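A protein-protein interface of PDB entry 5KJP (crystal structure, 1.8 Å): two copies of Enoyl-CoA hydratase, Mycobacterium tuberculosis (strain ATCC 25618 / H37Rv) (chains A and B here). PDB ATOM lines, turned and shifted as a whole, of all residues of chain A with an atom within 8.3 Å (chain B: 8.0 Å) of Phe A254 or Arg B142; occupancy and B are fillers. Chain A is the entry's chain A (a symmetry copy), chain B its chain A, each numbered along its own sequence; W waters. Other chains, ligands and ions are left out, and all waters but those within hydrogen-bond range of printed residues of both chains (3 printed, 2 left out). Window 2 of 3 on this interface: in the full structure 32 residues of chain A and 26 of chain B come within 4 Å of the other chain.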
ATOM      1  N   ALA A 206      22.357  -9.088  25.609  1.00  0.00           N
ATOM      2  CA  ALA A 206      21.437  -9.667  24.638  1.00  0.00           C
ATOM      3  C   ALA A 206      20.625 -10.799  25.260  1.00  0.00           C
ATOM      4  O   ALA A 206      19.632 -11.246  24.687  1.00  0.00           O
ATOM      5  CB  ALA A 206      22.192 -10.173  23.412  1.00  0.00           C
ATOM      6  N   ASN A 207      21.056 -11.265  26.428  1.00  0.00           N
ATOM      7  CA  ASN A 207      20.383 -12.376  27.085  1.00  0.00           C
ATOM      8  C   ASN A 207      19.358 -11.866  28.096  1.00  0.00           C
ATOM      9  O   ASN A 207      19.331 -10.677  28.401  1.00  0.00           O
ATOM     10  CB  ASN A 207      21.420 -13.295  27.734  1.00  0.00           C
ATOM     11  CG  ASN A 207      22.276 -14.004  26.693  1.00  0.00           C
ATOM     12  OD1 ASN A 207      21.847 -14.184  25.555  1.00  0.00           O
ATOM     13  ND2 ASN A 207      23.493 -14.391  27.071  1.00  0.00           N
ATOM     14  N   GLY A 208      18.498 -12.752  28.591  1.00  0.00           N
ATOM     15  CA  GLY A 208      17.402 -12.334  29.457  1.00  0.00           C
ATOM     16  C   GLY A 208      17.907 -11.706  30.741  1.00  0.00           C
ATOM     17  O   GLY A 208      18.618 -12.359  31.504  1.00  0.00           O
ATOM     18  N   PRO A 209      17.549 -10.434  30.990  1.00  0.00           N
ATOM     19  CA  PRO A 209      18.112  -9.704  32.137  1.00  0.00           C
ATOM     20  C   PRO A 209      17.806 -10.362  33.491  1.00  0.00           C
ATOM     21  O   PRO A 209      18.690 -10.431  34.345  1.00  0.00           O
ATOM     22  CB  PRO A 209      17.458  -8.319  32.030  1.00  0.00           C
ATOM     23  CG  PRO A 209      16.245  -8.521  31.170  1.00  0.00           C
ATOM     24  CD  PRO A 209      16.627  -9.601  30.201  1.00  0.00           C
ATOM     25  N   ALA A 211      17.227 -13.540  33.945  1.00  0.00           N
ATOM     26  CA  ALA A 211      17.942 -14.810  33.940  1.00  0.00           C
ATOM     27  C   ALA A 211      19.433 -14.589  34.182  1.00  0.00           C
ATOM     28  O   ALA A 211      20.068 -15.345  34.911  1.00  0.00           O
ATOM     29  CB  ALA A 211      17.708 -15.550  32.623  1.00  0.00           C
ATOM     30  N   VAL A 241      12.151 -16.519  37.878  1.00  0.00           N
ATOM     31  CA  VAL A 241      12.637 -16.434  36.508  1.00  0.00           C
ATOM     32  C   VAL A 241      11.739 -17.241  35.571  1.00  0.00           C
ATOM     33  O   VAL A 241      11.308 -16.751  34.520  1.00  0.00           O
ATOM     34  CB  VAL A 241      14.092 -16.933  36.390  1.00  0.00           C
ATOM     35  CG1 VAL A 241      14.540 -16.925  34.935  1.00  0.00           C
ATOM     36  CG2 VAL A 241      15.012 -16.061  37.240  1.00  0.00           C
ATOM     37  N   PHE A 242      11.442 -18.475  35.963  1.00  0.00           N
ATOM     38  CA  PHE A 242      10.666 -19.371  35.114  1.00  0.00           C
ATOM     39  C   PHE A 242       9.223 -18.914  34.902  1.00  0.00           C
ATOM     40  O   PHE A 242       8.593 -19.302  33.922  1.00  0.00           O
ATOM     41  CB  PHE A 242      10.689 -20.788  35.690  1.00  0.00           C
ATOM     42  CG  PHE A 242      11.863 -21.598  35.227  1.00  0.00           C
ATOM     43  CD1 PHE A 242      13.140 -21.302  35.671  1.00  0.00           C
ATOM     44  CD2 PHE A 242      11.693 -22.643  34.330  1.00  0.00           C
ATOM     45  CE1 PHE A 242      14.230 -22.037  35.237  1.00  0.00           C
ATOM     46  CE2 PHE A 242      12.778 -23.383  33.895  1.00  0.00           C
ATOM     47  CZ  PHE A 242      14.049 -23.080  34.351  1.00  0.00           C
ATOM     48  N   SER A 244       8.438 -15.622  34.767  1.00  0.00           N
ATOM     49  CA  SER A 244       8.502 -14.238  34.307  1.00  0.00           C
ATOM     50  C   SER A 244       7.916 -14.066  32.911  1.00  0.00           C
ATOM     51  O   SER A 244       7.802 -15.028  32.150  1.00  0.00           O
ATOM     52  CB  SER A 244       9.951 -13.739  34.316  1.00  0.00           C
ATOM     53  OG  SER A 244      10.752 -14.488  33.411  1.00  0.00           O
ATOM     54  N   ASN A 245       7.555 -12.832  32.576  1.00  0.00           N
ATOM     55  CA  ASN A 245       7.174 -12.505  31.210  1.00  0.00           C
ATOM     56  C   ASN A 245       8.292 -12.813  30.214  1.00  0.00           C
ATOM     57  O   ASN A 245       8.034 -13.237  29.085  1.00  0.00           O
ATOM     58  CB  ASN A 245       6.776 -11.034  31.109  1.00  0.00           C
ATOM     59  CG  ASN A 245       5.480 -10.737  31.832  1.00  0.00           C
ATOM     60  OD1 ASN A 245       4.526 -11.509  31.757  1.00  0.00           O
ATOM     61  ND2 ASN A 245       5.442  -9.620  32.546  1.00  0.00           N
ATOM     62  N   ASP A 246       9.533 -12.608  30.639  1.00  0.00           N
ATOM     63  CA  ASP A 246      10.670 -12.818  29.753  1.00  0.00           C
ATOM     64  C   ASP A 246      10.853 -14.292  29.420  1.00  0.00           C
ATOM     65  O   ASP A 246      11.347 -14.632  28.338  1.00  0.00           O
ATOM     66  CB  ASP A 246      11.952 -12.247  30.369  1.00  0.00           C
ATOM     67  CG  ASP A 246      12.107 -10.753  30.116  1.00  0.00           C
ATOM     68  OD1 ASP A 246      11.341 -10.194  29.293  1.00  0.00           O
ATOM     69  OD2 ASP A 246      12.998 -10.136  30.738  1.00  0.00           O
ATOM     70  N   ALA A 247      10.462 -15.168  30.341  1.00  0.00           N
ATOM     71  CA  ALA A 247      10.546 -16.604  30.088  1.00  0.00           C
ATOM     72  C   ALA A 247       9.602 -16.974  28.947  1.00  0.00           C
ATOM     73  O   ALA A 247       9.941 -17.789  28.085  1.00  0.00           O
ATOM     74  CB  ALA A 247      10.214 -17.406  31.352  1.00  0.00           C
ATOM     75  N   LYS A 248       8.423 -16.359  28.938  1.00  0.00           N
ATOM     76  CA  LYS A 248       7.459 -16.584  27.865  1.00  0.00           C
ATOM     77  C   LYS A 248       7.995 -16.029  26.549  1.00  0.00           C
ATOM     78  O   LYS A 248       7.968 -16.704  25.521  1.00  0.00           O
ATOM     79  CB  LYS A 248       6.110 -15.943  28.205  1.00  0.00           C
ATOM     80  CG  LYS A 248       5.093 -16.004  27.081  1.00  0.00           C
ATOM     81  CD  LYS A 248       3.776 -15.378  27.520  1.00  0.00           C
ATOM     82  CE  LYS A 248       2.786 -15.315  26.373  1.00  0.00           C
ATOM     83  NZ  LYS A 248       1.481 -14.752  26.832  1.00  0.00           N
ATOM     84  N   GLU A 249       8.483 -14.794  26.595  1.00  0.00           N
ATOM     85  CA  GLU A 249       9.004 -14.119  25.414  1.00  0.00           C
ATOM     86  C   GLU A 249      10.197 -14.872  24.824  1.00  0.00           C
ATOM     87  O   GLU A 249      10.337 -14.972  23.605  1.00  0.00           O
ATOM     88  CB  GLU A 249       9.396 -12.678  25.766  1.00  0.00           C
ATOM     89  CG  GLU A 249      10.184 -11.935  24.700  1.00  0.00           C
ATOM     90  CD  GLU A 249       9.387 -11.664  23.435  1.00  0.00           C
ATOM     91  OE1 GLU A 249       8.152 -11.867  23.431  1.00  0.00           O
ATOM     92  OE2 GLU A 249      10.005 -11.247  22.434  1.00  0.00           O
ATOM     93  N   GLY A 250      11.048 -15.408  25.694  1.00  0.00           N
ATOM     94  CA  GLY A 250      12.210 -16.155  25.258  1.00  0.00           C
ATOM     95  C   GLY A 250      11.808 -17.396  24.490  1.00  0.00           C
ATOM     96  O   GLY A 250      12.417 -17.733  23.473  1.00  0.00           O
ATOM     97  N   ALA A 251      10.765 -18.071  24.967  1.00  0.00           N
ATOM     98  CA  ALA A 251      10.290 -19.289  24.319  1.00  0.00           C
ATOM     99  C   ALA A 251       9.631 -18.968  22.977  1.00  0.00           C
ATOM    100  O   ALA A 251       9.842 -19.671  21.990  1.00  0.00           O
ATOM    101  CB  ALA A 251       9.319 -20.031  25.228  1.00  0.00           C
ATOM    102  N   ILE A 252       8.829 -17.906  22.957  1.00  0.00           N
ATOM    103  CA  ILE A 252       8.162 -17.460  21.740  1.00  0.00           C
ATOM    104  C   ILE A 252       9.178 -17.055  20.679  1.00  0.00           C
ATOM    105  O   ILE A 252       9.090 -17.478  19.522  1.00  0.00           O
ATOM    106  CB  ILE A 252       7.225 -16.263  22.012  1.00  0.00           C
ATOM    107  CG1 ILE A 252       6.033 -16.692  22.871  1.00  0.00           C
ATOM    108  CG2 ILE A 252       6.742 -15.655  20.706  1.00  0.00           C
ATOM    109  CD1 ILE A 252       5.068 -17.605  22.160  1.00  0.00           C
ATOM    110  N   ALA A 253      10.142 -16.233  21.086  1.00  0.00           N
ATOM    111  CA  ALA A 253      11.146 -15.709  20.168  1.00  0.00           C
ATOM    112  C   ALA A 253      11.965 -16.828  19.540  1.00  0.00           C
ATOM    113  O   ALA A 253      12.193 -16.835  18.330  1.00  0.00           O
ATOM    114  CB  ALA A 253      12.057 -14.734  20.888  1.00  0.00           C
ATOM    115  N   PHE A 254      12.395 -17.776  20.369  1.00  0.00           N
ATOM    116  CA  PHE A 254      13.167 -18.914  19.890  1.00  0.00           C
ATOM    117  C   PHE A 254      12.371 -19.734  18.874  1.00  0.00           C
ATOM    118  O   PHE A 254      12.893 -20.110  17.825  1.00  0.00           O
ATOM    119  CB  PHE A 254      13.601 -19.801  21.060  1.00  0.00           C
ATOM    120  CG  PHE A 254      14.775 -20.680  20.744  1.00  0.00           C
ATOM    121  CD1 PHE A 254      16.032 -20.385  21.247  1.00  0.00           C
ATOM    122  CD2 PHE A 254      14.630 -21.789  19.921  1.00  0.00           C
ATOM    123  CE1 PHE A 254      17.118 -21.189  20.952  1.00  0.00           C
ATOM    124  CE2 PHE A 254      15.715 -22.596  19.619  1.00  0.00           C
ATOM    125  CZ  PHE A 254      16.958 -22.297  20.138  1.00  0.00           C
ATOM    126  N   ALA A 255      11.109 -20.005  19.191  1.00  0.00           N
ATOM    127  CA  ALA A 255      10.249 -20.790  18.316  1.00  0.00           C
ATOM    128  C   ALA A 255      10.018 -20.080  16.986  1.00  0.00           C
ATOM    129  O   ALA A 255       9.793 -20.722  15.957  1.00  0.00           O
ATOM    130  CB  ALA A 255       8.914 -21.082  18.998  1.00  0.00           C
ATOM    131  N   GLU A 256      10.085 -18.752  17.008  1.00  0.00           N
ATOM    132  CA  GLU A 256       9.861 -17.960  15.805  1.00  0.00           C
ATOM    133  C   GLU A 256      11.178 -17.526  15.155  1.00  0.00           C
ATOM    134  O   GLU A 256      11.179 -16.734  14.214  1.00  0.00           O
ATOM    135  CB  GLU A 256       8.992 -16.743  16.132  1.00  0.00           C
ATOM    136  CG  GLU A 256       7.594 -17.121  16.612  1.00  0.00           C
ATOM    137  CD  GLU A 256       6.734 -15.917  16.966  1.00  0.00           C
ATOM    138  OE1 GLU A 256       7.268 -14.791  17.029  1.00  0.00           O
ATOM    139  OE2 GLU A 256       5.520 -16.104  17.179  1.00  0.00           O
ATOM    140  N   ARG A 257      12.288 -18.064  15.663  1.00  0.00           N
ATOM    141  CA  ARG A 257      13.631 -17.780  15.141  1.00  0.00           C
ATOM    142  C   ARG A 257      13.929 -16.292  14.988  1.00  0.00           C
ATOM    143  O   ARG A 257      14.428 -15.862  13.951  1.00  0.00           O
ATOM    144  CB  ARG A 257      13.842 -18.458  13.787  1.00  0.00           C
ATOM    145  CG  ARG A 257      13.754 -19.966  13.805  1.00  0.00           C
ATOM    146  CD  ARG A 257      14.136 -20.512  12.441  1.00  0.00           C
ATOM    147  NE  ARG A 257      13.730 -21.900  12.266  1.00  0.00           N
ATOM    148  CZ  ARG A 257      12.551 -22.271  11.779  1.00  0.00           C
ATOM    149  NH1 ARG A 257      11.659 -21.355  11.427  1.00  0.00           N
ATOM    150  NH2 ARG A 257      12.262 -23.559  11.649  1.00  0.00           N
ATOM    151  N   ARG A 258      13.617 -15.506  16.010  1.00  0.00           N
ATOM    152  CA  ARG A 258      13.910 -14.081  15.964  1.00  0.00           C
ATOM    153  C   ARG A 258      14.335 -13.590  17.339  1.00  0.00           C
ATOM    154  O   ARG A 258      14.247 -14.327  18.319  1.00  0.00           O
ATOM    155  CB  ARG A 258      12.699 -13.299  15.444  1.00  0.00           C
ATOM    156  CG  ARG A 258      11.371 -13.681  16.072  1.00  0.00           C
ATOM    157  CD  ARG A 258      11.091 -12.867  17.319  1.00  0.00           C
ATOM    158  NE  ARG A 258       9.743 -13.087  17.837  1.00  0.00           N
ATOM    159  CZ  ARG A 258       9.304 -12.592  18.990  1.00  0.00           C
ATOM    160  NH1 ARG A 258      10.109 -11.852  19.741  1.00  0.00           N
ATOM    161  NH2 ARG A 258       8.065 -12.836  19.390  1.00  0.00           N
ATOM    162  N   ARG A 259      14.802 -12.348  17.405  1.00  0.00           N
ATOM    163  CA  ARG A 259      15.328 -11.808  18.649  1.00  0.00           C
ATOM    164  C   ARG A 259      14.218 -11.580  19.659  1.00  0.00           C
ATOM    165  O   ARG A 259      13.155 -11.054  19.328  1.00  0.00           O
ATOM    166  CB  ARG A 259      16.091 -10.505  18.398  1.00  0.00           C
ATOM    167  CG  ARG A 259      17.391 -10.703  17.635  1.00  0.00           C
ATOM    168  CD  ARG A 259      18.042  -9.378  17.273  1.00  0.00           C
ATOM    169  NE  ARG A 259      19.189  -9.558  16.384  1.00  0.00           N
ATOM    170  CZ  ARG A 259      19.965  -8.566  15.960  1.00  0.00           C
ATOM    171  NH1 ARG A 259      19.724  -7.321  16.350  1.00  0.00           N
ATOM    172  NH2 ARG A 259      20.988  -8.816  15.153  1.00  0.00           N
ATOM    173  N   PRO A 260      14.454 -12.005  20.902  1.00  0.00           N
ATOM    174  CA  PRO A 260      13.518 -11.753  22.000  1.00  0.00           C
ATOM    175  C   PRO A 260      13.526 -10.290  22.419  1.00  0.00           C
ATOM    176  O   PRO A 260      14.583  -9.667  22.465  1.00  0.00           O
ATOM    177  CB  PRO A 260      14.046 -12.650  23.123  1.00  0.00           C
ATOM    178  CG  PRO A 260      15.494 -12.819  22.807  1.00  0.00           C
ATOM    179  CD  PRO A 260      15.591 -12.841  21.319  1.00  0.00           C
ATOM    180  N   TRP A 262      13.146  -8.354  25.448  1.00  0.00           N
ATOM    181  CA  TRP A 262      13.083  -8.490  26.895  1.00  0.00           C
ATOM    182  C   TRP A 262      12.406  -7.284  27.535  1.00  0.00           C
ATOM    183  O   TRP A 262      12.501  -6.169  27.024  1.00  0.00           O
ATOM    184  CB  TRP A 262      14.486  -8.653  27.489  1.00  0.00           C
ATOM    185  CG  TRP A 262      15.336  -9.747  26.895  1.00  0.00           C
ATOM    186  CD1 TRP A 262      16.560  -9.599  26.308  1.00  0.00           C
ATOM    187  CD2 TRP A 262      15.039 -11.152  26.850  1.00  0.00           C
ATOM    188  NE1 TRP A 262      17.044 -10.820  25.898  1.00  0.00           N
ATOM    189  CE2 TRP A 262      16.131 -11.789  26.219  1.00  0.00           C
ATOM    190  CE3 TRP A 262      13.962 -11.931  27.283  1.00  0.00           C
ATOM    191  CZ2 TRP A 262      16.176 -13.169  26.016  1.00  0.00           C
ATOM    192  CZ3 TRP A 262      14.007 -13.304  27.071  1.00  0.00           C
ATOM    193  CH2 TRP A 262      15.105 -13.904  26.442  1.00  0.00           C
ATOM    194  N   LEU B  78      12.582 -29.935  25.048  1.00  0.00           N
ATOM    195  CA  LEU B  78      11.665 -28.827  25.274  1.00  0.00           C
ATOM    196  C   LEU B  78      10.227 -29.140  24.862  1.00  0.00           C
ATOM    197  O   LEU B  78       9.286 -28.645  25.477  1.00  0.00           O
ATOM    198  CB  LEU B  78      12.160 -27.591  24.533  1.00  0.00           C
ATOM    199  CG  LEU B  78      13.565 -27.196  24.995  1.00  0.00           C
ATOM    200  CD1 LEU B  78      14.059 -26.015  24.217  1.00  0.00           C
ATOM    201  CD2 LEU B  78      13.572 -26.898  26.491  1.00  0.00           C
ATOM    202  N   LYS B  79      10.052 -29.952  23.825  1.00  0.00           N
ATOM    203  CA  LYS B  79       8.699 -30.314  23.397  1.00  0.00           C
ATOM    204  C   LYS B  79       8.038 -31.206  24.437  1.00  0.00           C
ATOM    205  O   LYS B  79       6.899 -30.966  24.841  1.00  0.00           O
ATOM    206  CB  LYS B  79       8.712 -31.018  22.039  1.00  0.00           C
ATOM    207  CG  LYS B  79       9.329 -30.212  20.914  1.00  0.00           C
ATOM    208  CD  LYS B  79       9.246 -30.987  19.610  1.00  0.00           C
ATOM    209  CE  LYS B  79      10.323 -30.549  18.638  1.00  0.00           C
ATOM    210  NZ  LYS B  79      11.685 -30.760  19.205  1.00  0.00           N
ATOM    211  N   PHE B  81       8.834 -31.459  27.521  1.00  0.00           N
ATOM    212  CA  PHE B  81       8.617 -30.585  28.666  1.00  0.00           C
ATOM    213  C   PHE B  81       7.370 -29.712  28.510  1.00  0.00           C
ATOM    214  O   PHE B  81       6.523 -29.676  29.404  1.00  0.00           O
ATOM    215  CB  PHE B  81       9.830 -29.691  28.892  1.00  0.00           C
ATOM    216  CG  PHE B  81       9.742 -28.871  30.143  1.00  0.00           C
ATOM    217  CD1 PHE B  81       9.736 -29.484  31.387  1.00  0.00           C
ATOM    218  CD2 PHE B  81       9.640 -27.490  30.079  1.00  0.00           C
ATOM    219  CE1 PHE B  81       9.645 -28.735  32.545  1.00  0.00           C
ATOM    220  CE2 PHE B  81       9.548 -26.735  31.234  1.00  0.00           C
ATOM    221  CZ  PHE B  81       9.550 -27.357  32.468  1.00  0.00           C
ATOM    222  N   ALA B 115      23.268 -27.481  27.538  1.00  0.00           N
ATOM    223  CA  ALA B 115      22.247 -27.209  28.549  1.00  0.00           C
ATOM    224  C   ALA B 115      22.150 -28.393  29.495  1.00  0.00           C
ATOM    225  O   ALA B 115      23.134 -28.740  30.150  1.00  0.00           O
ATOM    226  CB  ALA B 115      20.894 -26.906  27.889  1.00  0.00           C
ATOM    227  N   PRO B 138      23.391 -22.571  27.518  1.00  0.00           N
ATOM    228  CA  PRO B 138      22.820 -21.407  26.836  1.00  0.00           C
ATOM    229  C   PRO B 138      21.449 -20.977  27.379  1.00  0.00           C
ATOM    230  O   PRO B 138      20.765 -20.195  26.718  1.00  0.00           O
ATOM    231  CB  PRO B 138      22.700 -21.890  25.390  1.00  0.00           C
ATOM    232  CG  PRO B 138      22.444 -23.350  25.516  1.00  0.00           C
ATOM    233  CD  PRO B 138      23.214 -23.811  26.740  1.00  0.00           C
ATOM    234  N   GLU B 139      21.072 -21.457  28.564  1.00  0.00           N
ATOM    235  CA  GLU B 139      19.734 -21.208  29.107  1.00  0.00           C
ATOM    236  C   GLU B 139      19.355 -19.720  29.146  1.00  0.00           C
ATOM    237  O   GLU B 139      18.211 -19.365  28.851  1.00  0.00           O
ATOM    238  CB  GLU B 139      19.613 -21.819  30.513  1.00  0.00           C
ATOM    239  CG  GLU B 139      19.360 -23.344  30.536  1.00  0.00           C
ATOM    240  CD  GLU B 139      20.631 -24.194  30.409  1.00  0.00           C
ATOM    241  OE1 GLU B 139      21.648 -23.702  29.874  1.00  0.00           O
ATOM    242  OE2 GLU B 139      20.614 -25.368  30.851  1.00  0.00           O
ATOM    243  N   VAL B 140      20.307 -18.848  29.482  1.00  0.00           N
ATOM    244  CA  VAL B 140      19.993 -17.419  29.605  1.00  0.00           C
ATOM    245  C   VAL B 140      19.562 -16.801  28.276  1.00  0.00           C
ATOM    246  O   VAL B 140      18.893 -15.773  28.258  1.00  0.00           O
ATOM    247  CB  VAL B 140      21.191 -16.603  30.159  1.00  0.00           C
ATOM    248  CG1 VAL B 140      21.443 -16.939  31.631  1.00  0.00           C
ATOM    249  CG2 VAL B 140      22.434 -16.817  29.301  1.00  0.00           C
ATOM    250  N   LYS B 141      19.942 -17.426  27.166  1.00  0.00           N
ATOM    251  CA  LYS B 141      19.541 -16.932  25.846  1.00  0.00           C
ATOM    252  C   LYS B 141      18.025 -17.003  25.652  1.00  0.00           C
ATOM    253  O   LYS B 141      17.454 -16.237  24.868  1.00  0.00           O
ATOM    254  CB  LYS B 141      20.245 -17.722  24.740  1.00  0.00           C
ATOM    255  CG  LYS B 141      21.764 -17.569  24.719  1.00  0.00           C
ATOM    256  CD  LYS B 141      22.365 -18.275  23.508  1.00  0.00           C
ATOM    257  CE  LYS B 141      23.843 -17.956  23.348  1.00  0.00           C
ATOM    258  NZ  LYS B 141      24.497 -18.842  22.336  1.00  0.00           N
ATOM    259  N   ARG B 142      17.394 -17.935  26.365  1.00  0.00           N
ATOM    260  CA  ARG B 142      15.945 -18.122  26.328  1.00  0.00           C
ATOM    261  C   ARG B 142      15.287 -17.597  27.596  1.00  0.00           C
ATOM    262  O   ARG B 142      14.153 -17.971  27.914  1.00  0.00           O
ATOM    263  CB  ARG B 142      15.584 -19.600  26.152  1.00  0.00           C
ATOM    264  CG  ARG B 142      16.152 -20.257  24.912  1.00  0.00           C
ATOM    265  CD  ARG B 142      15.944 -21.766  24.965  1.00  0.00           C
ATOM    266  NE  ARG B 142      14.954 -22.211  23.992  1.00  0.00           N
ATOM    267  CZ  ARG B 142      13.688 -22.494  24.285  1.00  0.00           C
ATOM    268  NH1 ARG B 142      13.250 -22.386  25.534  1.00  0.00           N
ATOM    269  NH2 ARG B 142      12.861 -22.888  23.327  1.00  0.00           N
ATOM    270  N   GLY B 143      16.004 -16.747  28.325  1.00  0.00           N
ATOM    271  CA  GLY B 143      15.459 -16.115  29.510  1.00  0.00           C
ATOM    272  C   GLY B 143      15.247 -17.115  30.628  1.00  0.00           C
ATOM    273  O   GLY B 143      14.430 -16.887  31.523  1.00  0.00           O
ATOM    274  N   LEU B 144      15.980 -18.222  30.567  1.00  0.00           N
ATOM    275  CA  LEU B 144      15.934 -19.246  31.608  1.00  0.00           C
ATOM    276  C   LEU B 144      17.284 -19.403  32.298  1.00  0.00           C
ATOM    277  O   LEU B 144      18.250 -18.726  31.963  1.00  0.00           O
ATOM    278  CB  LEU B 144      15.484 -20.587  31.025  1.00  0.00           C
ATOM    279  CG  LEU B 144      14.055 -20.584  30.466  1.00  0.00           C
ATOM    280  CD1 LEU B 144      13.682 -21.965  29.935  1.00  0.00           C
ATOM    281  CD2 LEU B 144      13.055 -20.116  31.524  1.00  0.00           C
ATOM    282  N   VAL B 145      17.341 -20.309  33.263  1.00  0.00           N
ATOM    283  CA  VAL B 145      18.538 -20.504  34.067  1.00  0.00           C
ATOM    284  C   VAL B 145      18.879 -21.994  34.090  1.00  0.00           C
ATOM    285  O   VAL B 145      17.978 -22.830  34.127  1.00  0.00           O
ATOM    286  CB  VAL B 145      18.321 -19.960  35.498  1.00  0.00           C
ATOM    287  CG1 VAL B 145      19.505 -20.271  36.390  1.00  0.00           C
ATOM    288  CG2 VAL B 145      18.048 -18.453  35.458  1.00  0.00           C
HETATM  289  O   HOH W   1      13.478 -14.448  32.333  1.00  0.00           O
HETATM  290  O   HOH W   2      11.922 -19.608  27.926  1.00  0.00           O
HETATM  291  O   HOH W   3      14.960 -16.658  22.839  1.00  0.00           O
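Asn A207 touches Val B140. OD1 of Asn A207 touches CG of Lys B141, at 3.5 Å. CG1 of Val B140 touches O of Ala A211 (3.9 Å). Gly B143 touches Ala A211. Ala A211 touches Val B145. Val A241 touches Gly B143. Ala A247 touches Leu B144 (CB to CD2, 3.9 Å). Arg B142 touches Phe A254. CZ2 of Trp A262 touches O of Lys B141, 3.5 Å away. Trp A262 touches Arg B142.
No position is printed for both chains. Of the 16 pairs that touch across the chains among the printed residues, none has its exchanged pair printed and touching as well.
The backbone carbonyl oxygen of Val B140 is in hydrogen-bond range of the backbone NH of Gly A208, at 3.1 Å.
Hydrophobic or aromatic side chains of chain B within 4 Å of the printed part of chain A: Val B140, Leu B144 and Val B145. Hydrophobic or aromatic side chains of chain A that line the printed part of chain B: Ala A211, Val A241, Phe A242, Ala A247, Phe A254 and Trp A262. Among the printed residues, 16 pairs touch across the chains. Among the printed residues, no Asp or Glu carboxylate lies within 4 Å of a Lys or Arg side-chain nitrogen of the other chain.
The backbone carbonyl oxygen (O) of Glu B139 is in hydrogen-bond range of the backbone NH (N) of Leu B144, at 3.0 Å. O of Ala A206 sits at hydrogen-bond distance from NE1 of Trp A262 (2.9 Å). The backbone carbonyl oxygen (O) of Asn A207 sits close to the indole nitrogen (NE1) of Trp A262 (3.4 Å). OG of Ser A244 is in hydrogen-bond range of O of Val A241 (2.6 Å). The side-chain hydroxyl (OG) of Ser A244 is in hydrogen-bond range of the backbone NH (N) of Ala A247.
Water W2 bridges O of Ala A247 and O of Arg B142. Water W1 bridges O of Gly B143 (2.7 Å) and OG of Ser A244 (2.9 Å). Water W3 bridges the backbone carbonyl oxygen of Gly A250 (2.8 Å) and the backbone carbonyl oxygen of Lys B141 (3.2 Å).
Of the printed residues of chain B, Phe A254 touches Arg B142 (3.5 Å). Of the printed residues of chain A, Arg B142 touches Gly A250 (3.8 Å), Phe A254 (3.5 Å) and Trp A262 (3.9 Å). Ala A253 touches none of the printed residues of chain B. No residue of chain B comes within 4 Å of Ala A255. Printed residues of chain A within 4 Å of Gly B143: Ala A211 (3.5 Å), Val A241 (3.4 Å) and Trp A262 (3.5 Å). Of the printed residues of chain A, Leu B144 touches Ala A211 and Ala A247. Of the printed residues of chain B, Phe A242 touches Val B145 (3.9 Å). Printed residues of chain B within 4 Å of Val A241: Gly B143 (3.4 Å) and Val B145 (3.9 Å). Arg A259 touches none of the printed residues of chain B. The nearest printed residue of chain A that does not touch Arg B142 is Ala A247 (4.2 Å).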
